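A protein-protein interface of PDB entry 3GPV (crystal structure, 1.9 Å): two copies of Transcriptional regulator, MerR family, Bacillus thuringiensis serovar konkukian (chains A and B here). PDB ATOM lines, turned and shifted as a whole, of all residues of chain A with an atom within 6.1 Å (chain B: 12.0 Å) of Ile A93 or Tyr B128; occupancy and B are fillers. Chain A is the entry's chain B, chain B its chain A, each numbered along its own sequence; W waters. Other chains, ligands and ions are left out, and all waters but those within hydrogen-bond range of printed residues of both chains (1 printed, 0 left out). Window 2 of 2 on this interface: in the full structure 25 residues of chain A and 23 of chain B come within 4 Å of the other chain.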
ATOM      1  N   PHE A  82     -23.871  22.219  10.027  1.00  0.00           N
ATOM      2  CA  PHE A  82     -22.468  22.512   9.755  1.00  0.00           C
ATOM      3  C   PHE A  82     -22.122  23.886  10.326  1.00  0.00           C
ATOM      4  O   PHE A  82     -21.061  24.087  10.914  1.00  0.00           O
ATOM      5  CB  PHE A  82     -22.211  22.512   8.248  1.00  0.00           C
ATOM      6  CG  PHE A  82     -20.891  23.110   7.862  1.00  0.00           C
ATOM      7  CD1 PHE A  82     -19.707  22.422   8.094  1.00  0.00           C
ATOM      8  CD2 PHE A  82     -20.826  24.377   7.299  1.00  0.00           C
ATOM      9  CE1 PHE A  82     -18.471  22.986   7.774  1.00  0.00           C
ATOM     10  CE2 PHE A  82     -19.599  24.950   6.977  1.00  0.00           C
ATOM     11  CZ  PHE A  82     -18.417  24.251   7.215  1.00  0.00           C
ATOM     12  N   SER A  86     -19.676  24.893  13.397  1.00  0.00           N
ATOM     13  CA  SER A  86     -18.589  25.837  13.165  1.00  0.00           C
ATOM     14  C   SER A  86     -18.630  26.919  14.236  1.00  0.00           C
ATOM     15  O   SER A  86     -17.599  27.418  14.663  1.00  0.00           O
ATOM     16  CB  SER A  86     -18.720  26.477  11.777  1.00  0.00           C
ATOM     17  OG  SER A  86     -18.638  25.500  10.757  1.00  0.00           O
ATOM     18  N   GLY A  89     -17.155  26.084  17.868  1.00  0.00           N
ATOM     19  CA  GLY A  89     -15.713  26.073  18.059  1.00  0.00           C
ATOM     20  C   GLY A  89     -15.028  24.774  17.680  1.00  0.00           C
ATOM     21  O   GLY A  89     -15.675  23.832  17.229  1.00  0.00           O
ATOM     22  N   ASP A  90     -13.714  24.718  17.884  1.00  0.00           N
ATOM     23  CA  ASP A  90     -12.929  23.539  17.539  1.00  0.00           C
ATOM     24  C   ASP A  90     -13.272  22.279  18.319  1.00  0.00           C
ATOM     25  O   ASP A  90     -12.571  21.277  18.211  1.00  0.00           O
ATOM     26  CB  ASP A  90     -11.431  23.840  17.669  1.00  0.00           C
ATOM     27  CG  ASP A  90     -11.044  24.290  19.061  1.00  0.00           C
ATOM     28  OD1 ASP A  90     -11.651  25.259  19.562  1.00  0.00           O
ATOM     29  OD2 ASP A  90     -10.125  23.680  19.653  1.00  0.00           O
ATOM     30  N   SER A  91     -14.351  22.318  19.095  1.00  0.00           N
ATOM     31  CA  SER A  91     -14.761  21.143  19.853  1.00  0.00           C
ATOM     32  C   SER A  91     -15.578  20.228  18.940  1.00  0.00           C
ATOM     33  O   SER A  91     -15.940  19.114  19.318  1.00  0.00           O
ATOM     34  CB  SER A  91     -15.607  21.542  21.067  1.00  0.00           C
ATOM     35  OG  SER A  91     -16.915  21.926  20.684  1.00  0.00           O
ATOM     36  N   THR A  92     -15.869  20.712  17.736  1.00  0.00           N
ATOM     37  CA  THR A  92     -16.640  19.946  16.764  1.00  0.00           C
ATOM     38  C   THR A  92     -15.821  19.678  15.501  1.00  0.00           C
ATOM     39  O   THR A  92     -16.362  19.271  14.475  1.00  0.00           O
ATOM     40  CB  THR A  92     -17.910  20.699  16.349  1.00  0.00           C
ATOM     41  OG1 THR A  92     -17.541  21.918  15.694  1.00  0.00           O
ATOM     42  CG2 THR A  92     -18.762  21.020  17.565  1.00  0.00           C
ATOM     43  N   ILE A  93     -14.514  19.904  15.590  1.00  0.00           N
ATOM     44  CA  ILE A  93     -13.619  19.707  14.458  1.00  0.00           C
ATOM     45  C   ILE A  93     -13.765  18.332  13.808  1.00  0.00           C
ATOM     46  O   ILE A  93     -13.745  18.222  12.585  1.00  0.00           O
ATOM     47  CB  ILE A  93     -12.154  19.909  14.878  1.00  0.00           C
ATOM     48  CG1 ILE A  93     -11.234  19.802  13.658  1.00  0.00           C
ATOM     49  CG2 ILE A  93     -11.766  18.878  15.915  1.00  0.00           C
ATOM     50  CD1 ILE A  93     -11.331  20.972  12.702  1.00  0.00           C
ATOM     51  N   LEU A  94     -13.911  17.286  14.618  1.00  0.00           N
ATOM     52  CA  LEU A  94     -14.057  15.940  14.079  1.00  0.00           C
ATOM     53  C   LEU A  94     -15.407  15.776  13.389  1.00  0.00           C
ATOM     54  O   LEU A  94     -15.509  15.093  12.370  1.00  0.00           O
ATOM     55  CB  LEU A  94     -13.912  14.894  15.192  1.00  0.00           C
ATOM     56  CG  LEU A  94     -12.594  14.878  15.969  1.00  0.00           C
ATOM     57  CD1 LEU A  94     -12.602  13.689  16.908  1.00  0.00           C
ATOM     58  CD2 LEU A  94     -11.403  14.799  15.024  1.00  0.00           C
ATOM     59  N   HIS A  95     -16.440  16.400  13.948  1.00  0.00           N
ATOM     60  CA  HIS A  95     -17.779  16.319  13.371  1.00  0.00           C
ATOM     61  C   HIS A  95     -17.746  16.957  11.987  1.00  0.00           C
ATOM     62  O   HIS A  95     -18.144  16.354  10.991  1.00  0.00           O
ATOM     63  CB  HIS A  95     -18.797  17.087  14.221  1.00  0.00           C
ATOM     64  CG  HIS A  95     -18.711  16.808  15.690  1.00  0.00           C
ATOM     65  ND1 HIS A  95     -17.527  16.872  16.392  1.00  0.00           N
ATOM     66  CD2 HIS A  95     -19.675  16.534  16.600  1.00  0.00           C
ATOM     67  CE1 HIS A  95     -17.766  16.650  17.672  1.00  0.00           C
ATOM     68  NE2 HIS A  95     -19.061  16.443  17.825  1.00  0.00           N
ATOM     69  N   ARG A  96     -17.275  18.196  11.946  1.00  0.00           N
ATOM     70  CA  ARG A  96     -17.190  18.941  10.703  1.00  0.00           C
ATOM     71  C   ARG A  96     -16.305  18.249   9.681  1.00  0.00           C
ATOM     72  O   ARG A  96     -16.640  18.211   8.503  1.00  0.00           O
ATOM     73  CB  ARG A  96     -16.683  20.357  10.978  1.00  0.00           C
ATOM     74  CG  ARG A  96     -17.737  21.262  11.599  1.00  0.00           C
ATOM     75  CD  ARG A  96     -17.168  22.635  11.916  1.00  0.00           C
ATOM     76  NE  ARG A  96     -16.370  22.612  13.135  1.00  0.00           N
ATOM     77  CZ  ARG A  96     -15.198  23.220  13.272  1.00  0.00           C
ATOM     78  NH1 ARG A  96     -14.679  23.900  12.254  1.00  0.00           N
ATOM     79  NH2 ARG A  96     -14.546  23.155  14.425  1.00  0.00           N
ATOM     80  N   LEU A  97     -15.180  17.704  10.132  1.00  0.00           N
ATOM     81  CA  LEU A  97     -14.267  17.006   9.238  1.00  0.00           C
ATOM     82  C   LEU A  97     -15.006  15.830   8.620  1.00  0.00           C
ATOM     83  O   LEU A  97     -14.904  15.571   7.418  1.00  0.00           O
ATOM     84  CB  LEU A  97     -13.035  16.501   9.998  1.00  0.00           C
ATOM     85  CG  LEU A  97     -12.086  15.576   9.222  1.00  0.00           C
ATOM     86  CD1 LEU A  97     -11.537  16.288   8.003  1.00  0.00           C
ATOM     87  CD2 LEU A  97     -10.943  15.132  10.124  1.00  0.00           C
ATOM     88  N   LYS A  98     -15.762  15.126   9.450  1.00  0.00           N
ATOM     89  CA  LYS A  98     -16.526  13.992   8.974  1.00  0.00           C
ATOM     90  C   LYS A  98     -17.568  14.409   7.927  1.00  0.00           C
ATOM     91  O   LYS A  98     -17.675  13.774   6.877  1.00  0.00           O
ATOM     92  CB  LYS A  98     -17.199  13.283  10.157  1.00  0.00           C
ATOM     93  CG  LYS A  98     -18.147  12.138   9.784  1.00  0.00           C
ATOM     94  CD  LYS A  98     -17.546  11.165   8.762  1.00  0.00           C
ATOM     95  CE  LYS A  98     -16.252  10.536   9.247  1.00  0.00           C
ATOM     96  NZ  LYS A  98     -15.749   9.527   8.282  1.00  0.00           N
ATOM     97  N   MET A 100     -17.643  16.955   5.913  1.00  0.00           N
ATOM     98  CA  MET A 100     -17.015  17.326   4.655  1.00  0.00           C
ATOM     99  C   MET A 100     -16.578  16.092   3.893  1.00  0.00           C
ATOM    100  O   MET A 100     -16.766  16.019   2.684  1.00  0.00           O
ATOM    101  CB  MET A 100     -15.805  18.248   4.885  1.00  0.00           C
ATOM    102  CG  MET A 100     -16.181  19.645   5.287  1.00  0.00           C
ATOM    103  SD  MET A 100     -17.212  20.576   3.902  1.00  0.00           S
ATOM    104  CE  MET A 100     -18.925  20.448   4.765  1.00  0.00           C
ATOM    105  N   ASN B 117     -16.564  23.145  -6.854  1.00  0.00           N
ATOM    106  CA  ASN B 117     -17.079  22.947  -5.518  1.00  0.00           C
ATOM    107  C   ASN B 117     -16.356  21.815  -4.821  1.00  0.00           C
ATOM    108  O   ASN B 117     -16.124  21.881  -3.620  1.00  0.00           O
ATOM    109  CB  ASN B 117     -18.582  22.676  -5.564  1.00  0.00           C
ATOM    110  CG  ASN B 117     -19.375  23.896  -6.020  1.00  0.00           C
ATOM    111  OD1 ASN B 117     -19.033  25.027  -5.686  1.00  0.00           O
ATOM    112  ND2 ASN B 117     -20.442  23.664  -6.777  1.00  0.00           N
ATOM    113  N   LEU B 118     -15.997  20.775  -5.573  1.00  0.00           N
ATOM    114  CA  LEU B 118     -15.283  19.647  -4.987  1.00  0.00           C
ATOM    115  C   LEU B 118     -13.952  20.147  -4.421  1.00  0.00           C
ATOM    116  O   LEU B 118     -13.542  19.742  -3.340  1.00  0.00           O
ATOM    117  CB  LEU B 118     -15.023  18.565  -6.036  1.00  0.00           C
ATOM    118  CG  LEU B 118     -14.164  17.376  -5.568  1.00  0.00           C
ATOM    119  CD1 LEU B 118     -14.846  16.683  -4.407  1.00  0.00           C
ATOM    120  CD2 LEU B 118     -13.949  16.406  -6.721  1.00  0.00           C
ATOM    121  N   LYS B 119     -13.293  21.039  -5.157  1.00  0.00           N
ATOM    122  CA  LYS B 119     -12.015  21.588  -4.718  1.00  0.00           C
ATOM    123  C   LYS B 119     -12.147  22.358  -3.414  1.00  0.00           C
ATOM    124  O   LYS B 119     -11.292  22.243  -2.546  1.00  0.00           O
ATOM    125  CB  LYS B 119     -11.416  22.497  -5.795  1.00  0.00           C
ATOM    126  CG  LYS B 119      -9.916  22.718  -5.633  1.00  0.00           C
ATOM    127  CD  LYS B 119      -9.296  23.321  -6.890  1.00  0.00           C
ATOM    128  CE  LYS B 119      -7.776  23.403  -6.807  1.00  0.00           C
ATOM    129  NZ  LYS B 119      -7.176  23.923  -8.082  1.00  0.00           N
ATOM    130  N   LYS B 120     -13.211  23.141  -3.279  1.00  0.00           N
ATOM    131  CA  LYS B 120     -13.442  23.911  -2.058  1.00  0.00           C
ATOM    132  C   LYS B 120     -13.623  22.944  -0.887  1.00  0.00           C
ATOM    133  O   LYS B 120     -13.046  23.132   0.191  1.00  0.00           O
ATOM    134  CB  LYS B 120     -14.692  24.786  -2.203  1.00  0.00           C
ATOM    135  CG  LYS B 120     -14.553  25.919  -3.204  1.00  0.00           C
ATOM    136  CD  LYS B 120     -15.860  26.689  -3.349  1.00  0.00           C
ATOM    137  CE  LYS B 120     -15.733  27.790  -4.393  1.00  0.00           C
ATOM    138  NZ  LYS B 120     -17.040  28.463  -4.648  1.00  0.00           N
ATOM    139  N   ILE B 121     -14.422  21.905  -1.114  1.00  0.00           N
ATOM    140  CA  ILE B 121     -14.676  20.906  -0.094  1.00  0.00           C
ATOM    141  C   ILE B 121     -13.380  20.238   0.324  1.00  0.00           C
ATOM    142  O   ILE B 121     -13.112  20.074   1.511  1.00  0.00           O
ATOM    143  CB  ILE B 121     -15.635  19.808  -0.601  1.00  0.00           C
ATOM    144  CG1 ILE B 121     -17.018  20.404  -0.905  1.00  0.00           C
ATOM    145  CG2 ILE B 121     -15.739  18.689   0.432  1.00  0.00           C
ATOM    146  CD1 ILE B 121     -17.727  21.003   0.297  1.00  0.00           C
ATOM    147  N   GLN B 122     -12.580  19.840  -0.654  1.00  0.00           N
ATOM    148  CA  GLN B 122     -11.336  19.163  -0.363  1.00  0.00           C
ATOM    149  C   GLN B 122     -10.345  20.070   0.351  1.00  0.00           C
ATOM    150  O   GLN B 122      -9.601  19.613   1.218  1.00  0.00           O
ATOM    151  CB  GLN B 122     -10.736  18.602  -1.645  1.00  0.00           C
ATOM    152  CG  GLN B 122     -11.643  17.584  -2.320  1.00  0.00           C
ATOM    153  CD  GLN B 122     -10.990  16.928  -3.499  1.00  0.00           C
ATOM    154  OE1 GLN B 122     -10.317  17.588  -4.278  1.00  0.00           O
ATOM    155  NE2 GLN B 122     -11.196  15.624  -3.652  1.00  0.00           N
ATOM    156  N   GLN B 123     -10.330  21.350  -0.003  1.00  0.00           N
ATOM    157  CA  GLN B 123      -9.424  22.275   0.658  1.00  0.00           C
ATOM    158  C   GLN B 123      -9.845  22.396   2.126  1.00  0.00           C
ATOM    159  O   GLN B 123      -9.009  22.433   3.027  1.00  0.00           O
ATOM    160  CB  GLN B 123      -9.456  23.645  -0.032  1.00  0.00           C
ATOM    161  CG  GLN B 123      -8.910  23.615  -1.455  1.00  0.00           C
ATOM    162  CD  GLN B 123      -8.826  24.990  -2.093  1.00  0.00           C
ATOM    163  OE1 GLN B 123      -9.769  25.775  -2.027  1.00  0.00           O
ATOM    164  NE2 GLN B 123      -7.693  25.281  -2.730  1.00  0.00           N
ATOM    165  N   LYS B 124     -11.151  22.440   2.362  1.00  0.00           N
ATOM    166  CA  LYS B 124     -11.666  22.540   3.718  1.00  0.00           C
ATOM    167  C   LYS B 124     -11.220  21.312   4.504  1.00  0.00           C
ATOM    168  O   LYS B 124     -10.901  21.406   5.687  1.00  0.00           O
ATOM    169  CB  LYS B 124     -13.193  22.634   3.702  1.00  0.00           C
ATOM    170  CG  LYS B 124     -13.829  22.846   5.078  1.00  0.00           C
ATOM    171  CD  LYS B 124     -13.495  24.207   5.692  1.00  0.00           C
ATOM    172  CE  LYS B 124     -14.067  25.347   4.868  1.00  0.00           C
ATOM    173  NZ  LYS B 124     -13.823  26.700   5.448  1.00  0.00           N
ATOM    174  N   ILE B 125     -11.200  20.161   3.841  1.00  0.00           N
ATOM    175  CA  ILE B 125     -10.769  18.916   4.468  1.00  0.00           C
ATOM    176  C   ILE B 125      -9.291  19.001   4.850  1.00  0.00           C
ATOM    177  O   ILE B 125      -8.879  18.510   5.898  1.00  0.00           O
ATOM    178  CB  ILE B 125     -10.964  17.725   3.514  1.00  0.00           C
ATOM    179  CG1 ILE B 125     -12.460  17.465   3.333  1.00  0.00           C
ATOM    180  CG2 ILE B 125     -10.239  16.494   4.050  1.00  0.00           C
ATOM    181  CD1 ILE B 125     -12.777  16.497   2.234  1.00  0.00           C
ATOM    182  N   ALA B 126      -8.495  19.617   3.984  1.00  0.00           N
ATOM    183  CA  ALA B 126      -7.075  19.776   4.255  1.00  0.00           C
ATOM    184  C   ALA B 126      -6.924  20.684   5.474  1.00  0.00           C
ATOM    185  O   ALA B 126      -6.165  20.387   6.400  1.00  0.00           O
ATOM    186  CB  ALA B 126      -6.378  20.394   3.048  1.00  0.00           C
ATOM    187  N   LYS B 127      -7.673  21.784   5.467  1.00  0.00           N
ATOM    188  CA  LYS B 127      -7.640  22.754   6.553  1.00  0.00           C
ATOM    189  C   LYS B 127      -7.901  22.084   7.897  1.00  0.00           C
ATOM    190  O   LYS B 127      -7.220  22.370   8.883  1.00  0.00           O
ATOM    191  CB  LYS B 127      -8.674  23.851   6.312  1.00  0.00           C
ATOM    192  CG  LYS B 127      -8.558  25.032   7.267  1.00  0.00           C
ATOM    193  CD  LYS B 127      -9.498  26.151   6.871  1.00  0.00           C
ATOM    194  CE  LYS B 127      -9.349  27.347   7.785  1.00  0.00           C
ATOM    195  NZ  LYS B 127     -10.215  28.474   7.341  1.00  0.00           N
ATOM    196  N   TYR B 128      -8.886  21.193   7.936  1.00  0.00           N
ATOM    197  CA  TYR B 128      -9.208  20.492   9.170  1.00  0.00           C
ATOM    198  C   TYR B 128      -8.086  19.533   9.561  1.00  0.00           C
ATOM    199  O   TYR B 128      -7.598  19.644  10.705  1.00  0.00           O
ATOM    200  CB  TYR B 128     -10.519  19.713   9.027  1.00  0.00           C
ATOM    201  CG  TYR B 128     -11.756  20.572   8.859  1.00  0.00           C
ATOM    202  CD1 TYR B 128     -11.837  21.840   9.430  1.00  0.00           C
ATOM    203  CD2 TYR B 128     -12.869  20.092   8.171  1.00  0.00           C
ATOM    204  CE1 TYR B 128     -12.998  22.605   9.323  1.00  0.00           C
ATOM    205  CE2 TYR B 128     -14.030  20.848   8.062  1.00  0.00           C
ATOM    206  CZ  TYR B 128     -14.088  22.100   8.640  1.00  0.00           C
ATOM    207  OH  TYR B 128     -15.240  22.839   8.545  1.00  0.00           O
HETATM  208  O   HOH W   1     -16.151  25.189   9.779  1.00  0.00           O
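Among the printed residues, merely in contact across the chains: Phe A82 with Tyr B128, Ile A93 with Tyr B128, Arg A96 with Tyr B128, Leu A97 with Tyr B128, Met A100 with Ile B121, Met A100 with Lys B124, Met A100 with Ile B125 and Met A100 with Tyr B128.
O of Phe A82 is in hydrogen-bond range of OG of Ser A86 (2.8 Å). The guanidinium group (NE) of Arg A96 lies within hydrogen-bond range of the side-chain hydroxyl (OG1) of Thr A92 (2.9 Å). O of Gly A89 is in hydrogen-bond range of NH2 of Arg A96, at 3.1 Å.
Printed residues of chain B that touch a printed residue of chain A: Ile B121, Lys B124, Ile B125 and Tyr B128. Of the 13 printed residues of chain A, 5 touch a printed residue of chain B. Printed residues of chain A that touch a printed residue of chain B: Phe A82, Ile A93, Arg A96, Leu A97 and Met A100.
No position is printed for both chains. Of the 8 pairs that touch across the chains among the printed residues, none has its exchanged pair printed and touching as well.
Water W1 lies within hydrogen-bond range of the side-chain hydroxyl (OG) of Ser A86 (2.7 Å), the side-chain hydroxyl (OH) of Tyr B128 (2.8 Å) and the guanidinium group (NH1) of Arg A96 (3.2 Å).
Of the printed residues of chain B, Phe A82 touches Tyr B128 (3.3 Å). No residue of chain B comes within 4 Å of Gly A89. No residue of chain B comes within 4 Å of Asp A90. No residue of chain B comes within 4 Å of Ser A91. No residue of chain B comes within 4 Å of Thr A92. Ile A93 touches just one residue of chain B: Tyr B128 (3.4 Å). Of chain B, only Tyr B128 comes within 4 Å of Leu A97. Printed residues of chain A within 4 Å of Ile B121: Met A100. Printed residues of chain A within 4 Å of Lys B124: Met A100. Of the printed residues of chain A, Ile B125 touches Met A100 (3.8 Å). Ala B126 touches none of the printed residues of chain A. The nearest printed residue of chain B that does not touch Phe A82 is Lys B124 (5.1 Å).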
